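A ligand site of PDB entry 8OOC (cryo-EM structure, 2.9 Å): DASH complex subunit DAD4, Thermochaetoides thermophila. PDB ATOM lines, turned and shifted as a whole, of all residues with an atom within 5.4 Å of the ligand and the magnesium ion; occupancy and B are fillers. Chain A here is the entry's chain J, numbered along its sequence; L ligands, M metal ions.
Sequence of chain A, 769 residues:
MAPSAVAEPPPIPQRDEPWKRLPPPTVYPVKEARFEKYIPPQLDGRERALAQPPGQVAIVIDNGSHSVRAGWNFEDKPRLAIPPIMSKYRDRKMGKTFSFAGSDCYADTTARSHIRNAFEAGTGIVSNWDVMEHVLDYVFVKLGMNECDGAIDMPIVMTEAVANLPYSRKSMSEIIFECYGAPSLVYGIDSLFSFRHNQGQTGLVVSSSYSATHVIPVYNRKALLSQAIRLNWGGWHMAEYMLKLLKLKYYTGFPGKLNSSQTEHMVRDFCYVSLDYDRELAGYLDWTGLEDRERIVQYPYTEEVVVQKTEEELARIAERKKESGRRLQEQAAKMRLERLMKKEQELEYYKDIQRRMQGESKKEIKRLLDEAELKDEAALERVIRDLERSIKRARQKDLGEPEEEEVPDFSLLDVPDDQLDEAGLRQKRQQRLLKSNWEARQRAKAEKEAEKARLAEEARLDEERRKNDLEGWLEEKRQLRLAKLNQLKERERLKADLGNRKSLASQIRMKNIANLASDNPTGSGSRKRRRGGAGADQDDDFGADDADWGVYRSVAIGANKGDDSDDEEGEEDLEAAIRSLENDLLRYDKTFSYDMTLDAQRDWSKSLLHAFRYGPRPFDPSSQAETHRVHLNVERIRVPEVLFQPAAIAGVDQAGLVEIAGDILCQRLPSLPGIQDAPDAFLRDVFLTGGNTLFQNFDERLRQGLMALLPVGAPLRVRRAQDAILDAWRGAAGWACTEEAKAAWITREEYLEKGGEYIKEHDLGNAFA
The backbone NH (N) of Ser 211 lies within hydrogen-bond range of the side-chain hydroxyl (OG) of Ser 209 (3.3 Å). The guanidinium group (NH2) of Arg 69 is in salt-bridge range of the side-chain carboxylate (OD2) of Asp 62 (2.5 Å). N of Gly 235 lies within hydrogen-bond range of O of Ser 209 (2.9 Å). NH2 of Arg 268 lies within salt-bridge range of OE2 of Glu 264, at 2.7 Å. O of Tyr 210 sits at hydrogen-bond distance from N of Gly 235, 3.3 Å away. The backbone carbonyl oxygen (O) of Tyr 210 lies within hydrogen-bond range of the backbone NH (N) of Trp 236 (3.0 Å). The backbone carbonyl oxygen of Ser 208 is in hydrogen-bond range of the backbone NH of Asn 692. O of Ala 724 lies within hydrogen-bond range of N of Gly 690 (3.1 Å).
Arg 69 touches the magnesium ion (NH2 to MG, 3.99 Å). Two residues have an atom within 4 Å of the magnesium ion: Arg 69 and Asp 190.
O3 of the ligand sits at hydrogen-bond distance from N of Ser 211 (3.2 Å). An oxygen (O3) of the ligand lies within hydrogen-bond range of the side-chain hydroxyl of Ser 211, at 2.4 Å. An oxygen (O2) of the ligand lies within hydrogen-bond range of the backbone NH (N) of Ser 65. OG of Ser 65 sits at hydrogen-bond distance from O2 of the ligand, at 2.6 Å. The guanidinium group (NH1) of Arg 69 lies within salt-bridge range of an oxygen (O8) of the ligand (3.2 Å). The backbone NH of His 66 is in hydrogen-bond range of an oxygen (O5) of the ligand, 2.7 Å away. An oxygen (O3) of the ligand lies within hydrogen-bond range of the side-chain hydroxyl of Ser 209 (2.8 Å). An oxygen (O13) of the ligand sits at hydrogen-bond distance from the guanidinium group of Arg 268, 2.9 Å away. An oxygen (O7) of the ligand lies within hydrogen-bond range of the backbone NH (N) of Gly 691 (2.9 Å). An oxygen (O9) of the ligand lies within hydrogen-bond range of the backbone NH (N) of Tyr 210 (3.4 Å). An oxygen (O11) of the ligand sits at hydrogen-bond distance from the backbone NH (N) of Asn 692 (3.5 Å).
Residues that only touch the ligand: Gly 64 (3.2 Å), Leu 694 (3.4 Å), Gly 235 (3.4 Å), Glu 264 (3.6 Å), Gly 690 (3.6 Å), Ser 67 (3.6 Å), Asn 63 (3.7 Å), Ile 725 (3.7 Å) and Phe 695 (3.9 Å). Hydrophobic or aromatic side chains within 4 Å of the ligand: His 66, Tyr 210, Leu 694, Phe 695 and Ile 725. Of the 27 residues printed, 19 come within 4 Å of the ligand.
The magnesium ion is bound by OD2 of Asp 190, O1 of the ligand and O4 of the ligand.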
ATOM      1  N   ASP A  62     -23.098  -0.193 -10.837  1.00  0.00           N
ATOM      2  CA  ASP A  62     -22.952  -1.568 -11.287  1.00  0.00           C
ATOM      3  C   ASP A  62     -21.633  -1.711 -12.050  1.00  0.00           C
ATOM      4  O   ASP A  62     -21.480  -1.180 -13.148  1.00  0.00           O
ATOM      5  CB  ASP A  62     -24.141  -1.976 -12.164  1.00  0.00           C
ATOM      6  CG  ASP A  62     -24.014  -3.382 -12.723  1.00  0.00           C
ATOM      7  OD1 ASP A  62     -23.358  -4.217 -12.070  1.00  0.00           O
ATOM      8  OD2 ASP A  62     -24.585  -3.640 -13.801  1.00  0.00           O
ATOM      9  N   ASN A  63     -20.691  -2.442 -11.457  1.00  0.00           N
ATOM     10  CA  ASN A  63     -19.376  -2.678 -12.030  1.00  0.00           C
ATOM     11  C   ASN A  63     -19.417  -3.681 -13.176  1.00  0.00           C
ATOM     12  O   ASN A  63     -18.806  -4.751 -13.084  1.00  0.00           O
ATOM     13  CB  ASN A  63     -18.394  -3.174 -10.970  1.00  0.00           C
ATOM     14  CG  ASN A  63     -18.072  -2.125  -9.940  1.00  0.00           C
ATOM     15  OD1 ASN A  63     -18.005  -0.933 -10.245  1.00  0.00           O
ATOM     16  ND2 ASN A  63     -17.833  -2.558  -8.707  1.00  0.00           N
ATOM     17  N   GLY A  64     -20.128  -3.359 -14.247  1.00  0.00           N
ATOM     18  CA  GLY A  64     -20.127  -4.241 -15.405  1.00  0.00           C
ATOM     19  C   GLY A  64     -18.788  -4.215 -16.119  1.00  0.00           C
ATOM     20  O   GLY A  64     -18.271  -3.148 -16.470  1.00  0.00           O
ATOM     21  N   SER A  65     -18.210  -5.406 -16.316  1.00  0.00           N
ATOM     22  CA  SER A  65     -16.982  -5.533 -17.094  1.00  0.00           C
ATOM     23  C   SER A  65     -17.153  -5.072 -18.529  1.00  0.00           C
ATOM     24  O   SER A  65     -16.180  -4.675 -19.176  1.00  0.00           O
ATOM     25  CB  SER A  65     -16.489  -6.983 -17.058  1.00  0.00           C
ATOM     26  OG  SER A  65     -16.411  -7.466 -15.732  1.00  0.00           O
ATOM     27  N   HIS A  66     -18.370  -5.138 -19.054  1.00  0.00           N
ATOM     28  CA  HIS A  66     -18.668  -4.479 -20.318  1.00  0.00           C
ATOM     29  C   HIS A  66     -18.961  -2.989 -20.130  1.00  0.00           C
ATOM     30  O   HIS A  66     -18.554  -2.167 -20.953  1.00  0.00           O
ATOM     31  CB  HIS A  66     -19.846  -5.172 -21.005  1.00  0.00           C
ATOM     32  CG  HIS A  66     -20.246  -4.549 -22.305  1.00  0.00           C
ATOM     33  ND1 HIS A  66     -19.409  -4.520 -23.407  1.00  0.00           N
ATOM     34  CD2 HIS A  66     -21.389  -3.938 -22.695  1.00  0.00           C
ATOM     35  CE1 HIS A  66     -20.021  -3.920 -24.411  1.00  0.00           C
ATOM     36  NE2 HIS A  66     -21.219  -3.552 -24.006  1.00  0.00           N
ATOM     37  N   SER A  67     -19.667  -2.627 -19.057  1.00  0.00           N
ATOM     38  CA  SER A  67     -20.096  -1.240 -18.880  1.00  0.00           C
ATOM     39  C   SER A  67     -20.322  -0.993 -17.390  1.00  0.00           C
ATOM     40  O   SER A  67     -21.212  -1.604 -16.788  1.00  0.00           O
ATOM     41  CB  SER A  67     -21.365  -0.960 -19.675  1.00  0.00           C
ATOM     42  OG  SER A  67     -21.759   0.396 -19.548  1.00  0.00           O
ATOM     43  N   ARG A  69     -22.106   1.014 -14.897  1.00  0.00           N
ATOM     44  CA  ARG A  69     -23.357   1.765 -14.901  1.00  0.00           C
ATOM     45  C   ARG A  69     -23.539   2.455 -13.553  1.00  0.00           C
ATOM     46  O   ARG A  69     -23.465   1.801 -12.505  1.00  0.00           O
ATOM     47  CB  ARG A  69     -24.532   0.842 -15.212  1.00  0.00           C
ATOM     48  CG  ARG A  69     -24.511   0.297 -16.618  1.00  0.00           C
ATOM     49  CD  ARG A  69     -25.370  -0.952 -16.745  1.00  0.00           C
ATOM     50  NE  ARG A  69     -24.721  -2.095 -16.117  1.00  0.00           N
ATOM     51  CZ  ARG A  69     -24.267  -3.151 -16.780  1.00  0.00           C
ATOM     52  NH1 ARG A  69     -24.349  -3.232 -18.102  1.00  0.00           N
ATOM     53  NH2 ARG A  69     -23.710  -4.147 -16.099  1.00  0.00           N
ATOM     54  N   PHE A 119     -10.487  -4.606 -15.536  1.00  0.00           N
ATOM     55  CA  PHE A 119     -10.700  -6.015 -15.248  1.00  0.00           C
ATOM     56  C   PHE A 119      -9.590  -6.872 -15.863  1.00  0.00           C
ATOM     57  O   PHE A 119      -9.021  -6.529 -16.897  1.00  0.00           O
ATOM     58  CB  PHE A 119     -12.066  -6.482 -15.751  1.00  0.00           C
ATOM     59  CG  PHE A 119     -13.218  -5.882 -15.010  1.00  0.00           C
ATOM     60  CD1 PHE A 119     -13.735  -4.643 -15.360  1.00  0.00           C
ATOM     61  CD2 PHE A 119     -13.816  -6.567 -13.961  1.00  0.00           C
ATOM     62  CE1 PHE A 119     -14.805  -4.099 -14.677  1.00  0.00           C
ATOM     63  CE2 PHE A 119     -14.880  -6.031 -13.281  1.00  0.00           C
ATOM     64  CZ  PHE A 119     -15.378  -4.800 -13.639  1.00  0.00           C
ATOM     65  N   GLY A 124     -14.329 -11.837 -14.106  1.00  0.00           N
ATOM     66  CA  GLY A 124     -15.339 -11.036 -13.435  1.00  0.00           C
ATOM     67  C   GLY A 124     -14.811 -10.110 -12.375  1.00  0.00           C
ATOM     68  O   GLY A 124     -15.594  -9.369 -11.771  1.00  0.00           O
ATOM     69  N   ASP A 190     -24.927  -8.624  -8.816  1.00  0.00           N
ATOM     70  CA  ASP A 190     -25.722  -7.911  -9.816  1.00  0.00           C
ATOM     71  C   ASP A 190     -26.889  -8.746 -10.330  1.00  0.00           C
ATOM     72  O   ASP A 190     -27.994  -8.232 -10.509  1.00  0.00           O
ATOM     73  CB  ASP A 190     -24.819  -7.462 -10.976  1.00  0.00           C
ATOM     74  CG  ASP A 190     -24.339  -8.624 -11.833  1.00  0.00           C
ATOM     75  OD1 ASP A 190     -24.328  -9.772 -11.345  1.00  0.00           O
ATOM     76  OD2 ASP A 190     -23.972  -8.375 -13.009  1.00  0.00           O
ATOM     77  N   SER A 208     -25.916 -14.983 -17.804  1.00  0.00           N
ATOM     78  CA  SER A 208     -24.780 -14.944 -18.716  1.00  0.00           C
ATOM     79  C   SER A 208     -24.395 -13.505 -18.979  1.00  0.00           C
ATOM     80  O   SER A 208     -25.212 -12.715 -19.462  1.00  0.00           O
ATOM     81  CB  SER A 208     -25.101 -15.665 -20.035  1.00  0.00           C
ATOM     82  OG  SER A 208     -25.352 -17.033 -19.811  1.00  0.00           O
ATOM     83  N   SER A 209     -23.150 -13.171 -18.659  1.00  0.00           N
ATOM     84  CA  SER A 209     -22.651 -11.804 -18.608  1.00  0.00           C
ATOM     85  C   SER A 209     -21.532 -11.642 -19.633  1.00  0.00           C
ATOM     86  O   SER A 209     -21.306 -12.509 -20.474  1.00  0.00           O
ATOM     87  CB  SER A 209     -22.188 -11.470 -17.182  1.00  0.00           C
ATOM     88  OG  SER A 209     -21.053 -12.231 -16.830  1.00  0.00           O
ATOM     89  N   TYR A 210     -20.842 -10.505 -19.554  1.00  0.00           N
ATOM     90  CA  TYR A 210     -19.589 -10.360 -20.288  1.00  0.00           C
ATOM     91  C   TYR A 210     -18.523 -11.328 -19.790  1.00  0.00           C
ATOM     92  O   TYR A 210     -17.854 -11.990 -20.578  1.00  0.00           O
ATOM     93  CB  TYR A 210     -19.088  -8.912 -20.174  1.00  0.00           C
ATOM     94  CG  TYR A 210     -18.074  -8.513 -21.216  1.00  0.00           C
ATOM     95  CD1 TYR A 210     -18.440  -8.327 -22.543  1.00  0.00           C
ATOM     96  CD2 TYR A 210     -16.749  -8.290 -20.872  1.00  0.00           C
ATOM     97  CE1 TYR A 210     -17.509  -7.978 -23.501  1.00  0.00           C
ATOM     98  CE2 TYR A 210     -15.812  -7.916 -21.815  1.00  0.00           C
ATOM     99  CZ  TYR A 210     -16.201  -7.765 -23.134  1.00  0.00           C
ATOM    100  OH  TYR A 210     -15.281  -7.370 -24.066  1.00  0.00           O
ATOM    101  N   SER A 211     -18.359 -11.425 -18.471  1.00  0.00           N
ATOM    102  CA  SER A 211     -17.244 -12.196 -17.934  1.00  0.00           C
ATOM    103  C   SER A 211     -17.515 -13.694 -17.900  1.00  0.00           C
ATOM    104  O   SER A 211     -16.632 -14.491 -18.215  1.00  0.00           O
ATOM    105  CB  SER A 211     -16.894 -11.695 -16.532  1.00  0.00           C
ATOM    106  OG  SER A 211     -17.986 -11.882 -15.638  1.00  0.00           O
ATOM    107  N   ALA A 212     -18.725 -14.104 -17.512  1.00  0.00           N
ATOM    108  CA  ALA A 212     -18.946 -15.500 -17.176  1.00  0.00           C
ATOM    109  C   ALA A 212     -20.438 -15.799 -17.239  1.00  0.00           C
ATOM    110  O   ALA A 212     -21.262 -14.943 -17.554  1.00  0.00           O
ATOM    111  CB  ALA A 212     -18.375 -15.836 -15.793  1.00  0.00           C
ATOM    112  N   GLY A 235     -19.951 -13.137 -22.920  1.00  0.00           N
ATOM    113  CA  GLY A 235     -19.917 -12.294 -24.098  1.00  0.00           C
ATOM    114  C   GLY A 235     -18.519 -11.880 -24.524  1.00  0.00           C
ATOM    115  O   GLY A 235     -18.297 -11.564 -25.685  1.00  0.00           O
ATOM    116  N   TRP A 236     -17.577 -11.861 -23.586  1.00  0.00           N
ATOM    117  CA  TRP A 236     -16.176 -11.652 -23.948  1.00  0.00           C
ATOM    118  C   TRP A 236     -15.631 -12.841 -24.723  1.00  0.00           C
ATOM    119  O   TRP A 236     -15.095 -12.682 -25.828  1.00  0.00           O
ATOM    120  CB  TRP A 236     -15.341 -11.435 -22.685  1.00  0.00           C
ATOM    121  CG  TRP A 236     -13.892 -11.153 -22.977  1.00  0.00           C
ATOM    122  CD1 TRP A 236     -13.346  -9.966 -23.359  1.00  0.00           C
ATOM    123  CD2 TRP A 236     -12.816 -12.100 -22.967  1.00  0.00           C
ATOM    124  NE1 TRP A 236     -12.002 -10.101 -23.550  1.00  0.00           N
ATOM    125  CE2 TRP A 236     -11.649 -11.400 -23.321  1.00  0.00           C
ATOM    126  CE3 TRP A 236     -12.726 -13.470 -22.685  1.00  0.00           C
ATOM    127  CZ2 TRP A 236     -10.405 -12.022 -23.399  1.00  0.00           C
ATOM    128  CZ3 TRP A 236     -11.488 -14.084 -22.760  1.00  0.00           C
ATOM    129  CH2 TRP A 236     -10.341 -13.360 -23.113  1.00  0.00           C
ATOM    130  N   GLU A 264     -17.454  -8.639 -31.351  1.00  0.00           N
ATOM    131  CA  GLU A 264     -18.513  -8.389 -30.373  1.00  0.00           C
ATOM    132  C   GLU A 264     -19.813  -7.937 -31.039  1.00  0.00           C
ATOM    133  O   GLU A 264     -20.884  -8.474 -30.754  1.00  0.00           O
ATOM    134  CB  GLU A 264     -18.041  -7.352 -29.354  1.00  0.00           C
ATOM    135  CG  GLU A 264     -19.085  -6.928 -28.346  1.00  0.00           C
ATOM    136  CD  GLU A 264     -18.712  -5.631 -27.639  1.00  0.00           C
ATOM    137  OE1 GLU A 264     -17.628  -5.588 -27.031  1.00  0.00           O
ATOM    138  OE2 GLU A 264     -19.506  -4.668 -27.699  1.00  0.00           O
ATOM    139  N   VAL A 267     -21.295 -10.903 -33.080  1.00  0.00           N
ATOM    140  CA  VAL A 267     -22.006 -11.841 -32.205  1.00  0.00           C
ATOM    141  C   VAL A 267     -23.362 -11.283 -31.804  1.00  0.00           C
ATOM    142  O   VAL A 267     -24.393 -11.972 -31.879  1.00  0.00           O
ATOM    143  CB  VAL A 267     -21.155 -12.182 -30.973  1.00  0.00           C
ATOM    144  CG1 VAL A 267     -21.993 -12.891 -29.931  1.00  0.00           C
ATOM    145  CG2 VAL A 267     -19.964 -13.046 -31.378  1.00  0.00           C
ATOM    146  N   ARG A 268     -23.400 -10.024 -31.360  1.00  0.00           N
ATOM    147  CA  ARG A 268     -24.649  -9.377 -30.997  1.00  0.00           C
ATOM    148  C   ARG A 268     -25.653  -9.349 -32.141  1.00  0.00           C
ATOM    149  O   ARG A 268     -26.824  -9.710 -31.964  1.00  0.00           O
ATOM    150  CB  ARG A 268     -24.365  -7.956 -30.500  1.00  0.00           C
ATOM    151  CG  ARG A 268     -25.567  -7.270 -29.883  1.00  0.00           C
ATOM    152  CD  ARG A 268     -25.246  -5.851 -29.461  1.00  0.00           C
ATOM    153  NE  ARG A 268     -24.148  -5.816 -28.497  1.00  0.00           N
ATOM    154  CZ  ARG A 268     -23.108  -5.006 -28.575  1.00  0.00           C
ATOM    155  NH1 ARG A 268     -23.030  -4.057 -29.502  1.00  0.00           N
ATOM    156  NH2 ARG A 268     -22.124  -5.121 -27.683  1.00  0.00           N
ATOM    157  N   GLY A 690     -28.630 -10.892 -17.424  1.00  0.00           N
ATOM    158  CA  GLY A 690     -27.390 -10.539 -18.101  1.00  0.00           C
ATOM    159  C   GLY A 690     -27.505 -10.545 -19.609  1.00  0.00           C
ATOM    160  O   GLY A 690     -28.261 -11.319 -20.195  1.00  0.00           O
ATOM    161  N   GLY A 691     -26.746  -9.651 -20.252  1.00  0.00           N
ATOM    162  CA  GLY A 691     -26.926  -9.383 -21.671  1.00  0.00           C
ATOM    163  C   GLY A 691     -26.644 -10.574 -22.568  1.00  0.00           C
ATOM    164  O   GLY A 691     -27.291 -10.737 -23.601  1.00  0.00           O
ATOM    165  N   ASN A 692     -25.671 -11.404 -22.201  1.00  0.00           N
ATOM    166  CA  ASN A 692     -25.298 -12.544 -23.023  1.00  0.00           C
ATOM    167  C   ASN A 692     -26.374 -13.635 -23.073  1.00  0.00           C
ATOM    168  O   ASN A 692     -26.207 -14.612 -23.809  1.00  0.00           O
ATOM    169  CB  ASN A 692     -23.966 -13.107 -22.501  1.00  0.00           C
ATOM    170  CG  ASN A 692     -23.435 -14.252 -23.336  1.00  0.00           C
ATOM    171  OD1 ASN A 692     -23.218 -15.351 -22.836  1.00  0.00           O
ATOM    172  ND2 ASN A 692     -23.222 -13.995 -24.617  1.00  0.00           N
ATOM    173  N   LEU A 694     -29.310 -12.721 -24.239  1.00  0.00           N
ATOM    174  CA  LEU A 694     -30.282 -12.100 -25.141  1.00  0.00           C
ATOM    175  C   LEU A 694     -30.381 -12.778 -26.497  1.00  0.00           C
ATOM    176  O   LEU A 694     -31.108 -12.265 -27.365  1.00  0.00           O
ATOM    177  CB  LEU A 694     -29.952 -10.621 -25.325  1.00  0.00           C
ATOM    178  CG  LEU A 694     -30.319  -9.703 -24.166  1.00  0.00           C
ATOM    179  CD1 LEU A 694     -29.684  -8.342 -24.334  1.00  0.00           C
ATOM    180  CD2 LEU A 694     -31.822  -9.584 -24.064  1.00  0.00           C
ATOM    181  N   PHE A 695     -29.691 -13.888 -26.735  1.00  0.00           N
ATOM    182  CA  PHE A 695     -29.793 -14.558 -28.024  1.00  0.00           C
ATOM    183  C   PHE A 695     -31.208 -15.059 -28.278  1.00  0.00           C
ATOM    184  O   PHE A 695     -31.932 -15.442 -27.362  1.00  0.00           O
ATOM    185  CB  PHE A 695     -28.802 -15.723 -28.101  1.00  0.00           C
ATOM    186  CG  PHE A 695     -27.375 -15.309 -27.990  1.00  0.00           C
ATOM    187  CD1 PHE A 695     -26.783 -14.584 -29.017  1.00  0.00           C
ATOM    188  CD2 PHE A 695     -26.610 -15.633 -26.881  1.00  0.00           C
ATOM    189  CE1 PHE A 695     -25.466 -14.194 -28.925  1.00  0.00           C
ATOM    190  CE2 PHE A 695     -25.296 -15.240 -26.799  1.00  0.00           C
ATOM    191  CZ  PHE A 695     -24.725 -14.521 -27.821  1.00  0.00           C
ATOM    192  N   ALA A 724     -32.298  -7.118 -19.849  1.00  0.00           N
ATOM    193  CA  ALA A 724     -31.230  -8.013 -19.417  1.00  0.00           C
ATOM    194  C   ALA A 724     -30.029  -7.306 -18.807  1.00  0.00           C
ATOM    195  O   ALA A 724     -29.258  -7.963 -18.106  1.00  0.00           O
ATOM    196  CB  ALA A 724     -30.769  -8.873 -20.596  1.00  0.00           C
ATOM    197  N   ILE A 725     -29.828  -6.003 -19.034  1.00  0.00           N
ATOM    198  CA  ILE A 725     -28.595  -5.334 -18.635  1.00  0.00           C
ATOM    199  C   ILE A 725     -28.839  -4.258 -17.575  1.00  0.00           C
ATOM    200  O   ILE A 725     -28.153  -4.222 -16.553  1.00  0.00           O
ATOM    201  CB  ILE A 725     -27.847  -4.748 -19.856  1.00  0.00           C
ATOM    202  CG1 ILE A 725     -28.718  -3.771 -20.650  1.00  0.00           C
ATOM    203  CG2 ILE A 725     -27.358  -5.862 -20.768  1.00  0.00           C
ATOM    204  CD1 ILE A 725     -27.990  -3.091 -21.788  1.00  0.00           C
HETATM  205  P1  LIG L   1     -20.105  -8.705 -15.462  1.00  0.00           P
HETATM  206  O1  LIG L   1     -21.185  -8.679 -14.451  1.00  0.00           O
HETATM  207  O2  LIG L   1     -18.902  -7.827 -15.096  1.00  0.00           O
HETATM  208  O3  LIG L   1     -19.624 -10.103 -15.815  1.00  0.00           O
HETATM  209  P2  LIG L   1     -21.581  -6.953 -17.387  1.00  0.00           P
HETATM  210  O4  LIG L   1     -22.490  -6.470 -16.335  1.00  0.00           O
HETATM  211  O5  LIG L   1     -20.703  -5.905 -18.042  1.00  0.00           O
HETATM  212  O6  LIG L   1     -20.624  -8.099 -16.841  1.00  0.00           O
HETATM  213  P3  LIG L   1     -23.712  -7.468 -19.363  1.00  0.00           P
HETATM  214  O7  LIG L   1     -24.882  -8.047 -18.667  1.00  0.00           O
HETATM  215  O8  LIG L   1     -23.817  -5.969 -19.628  1.00  0.00           O
HETATM  216  O9  LIG L   1     -22.374  -7.688 -18.551  1.00  0.00           O
HETATM  217  O10 LIG L   1     -23.404  -8.185 -20.731  1.00  0.00           O
HETATM  218  C1  LIG L   1     -22.867  -7.461 -21.850  1.00  0.00           C
HETATM  219  C2  LIG L   1     -22.597  -8.448 -22.968  1.00  0.00           C
HETATM  220  O11 LIG L   1     -23.844  -8.800 -23.602  1.00  0.00           O
HETATM  221  C3  LIG L   1     -21.666  -7.950 -24.069  1.00  0.00           C
HETATM  222  O12 LIG L   1     -20.766  -8.979 -24.471  1.00  0.00           O
HETATM  223  C4  LIG L   1     -22.627  -7.580 -25.200  1.00  0.00           C
HETATM  224  O13 LIG L   1     -22.030  -7.712 -26.482  1.00  0.00           O
HETATM  225  C5  LIG L   1     -23.717  -8.636 -25.002  1.00  0.00           C
HETATM  226  N1  LIG L   1     -25.006  -8.269 -25.555  1.00  0.00           N
HETATM  227  C6  LIG L   1     -25.660  -7.069 -25.420  1.00  0.00           C
HETATM  228  N2  LIG L   1     -26.814  -7.013 -26.036  1.00  0.00           N
HETATM  229  C7  LIG L   1     -26.935  -8.261 -26.627  1.00  0.00           C
HETATM  230  C8  LIG L   1     -27.935  -8.845 -27.419  1.00  0.00           C
HETATM  231  N3  LIG L   1     -29.061  -8.222 -27.778  1.00  0.00           N
HETATM  232  N4  LIG L   1     -27.745 -10.115 -27.843  1.00  0.00           N
HETATM  233  C9  LIG L   1     -26.635 -10.750 -27.483  1.00  0.00           C
HETATM  234  N5  LIG L   1     -25.613 -10.306 -26.733  1.00  0.00           N
HETATM  235  C10 LIG L   1     -25.833  -9.048 -26.336  1.00  0.00           C
HETATM  236 MG    MG M   1     -23.094  -7.875 -14.810  1.00  0.00          MG
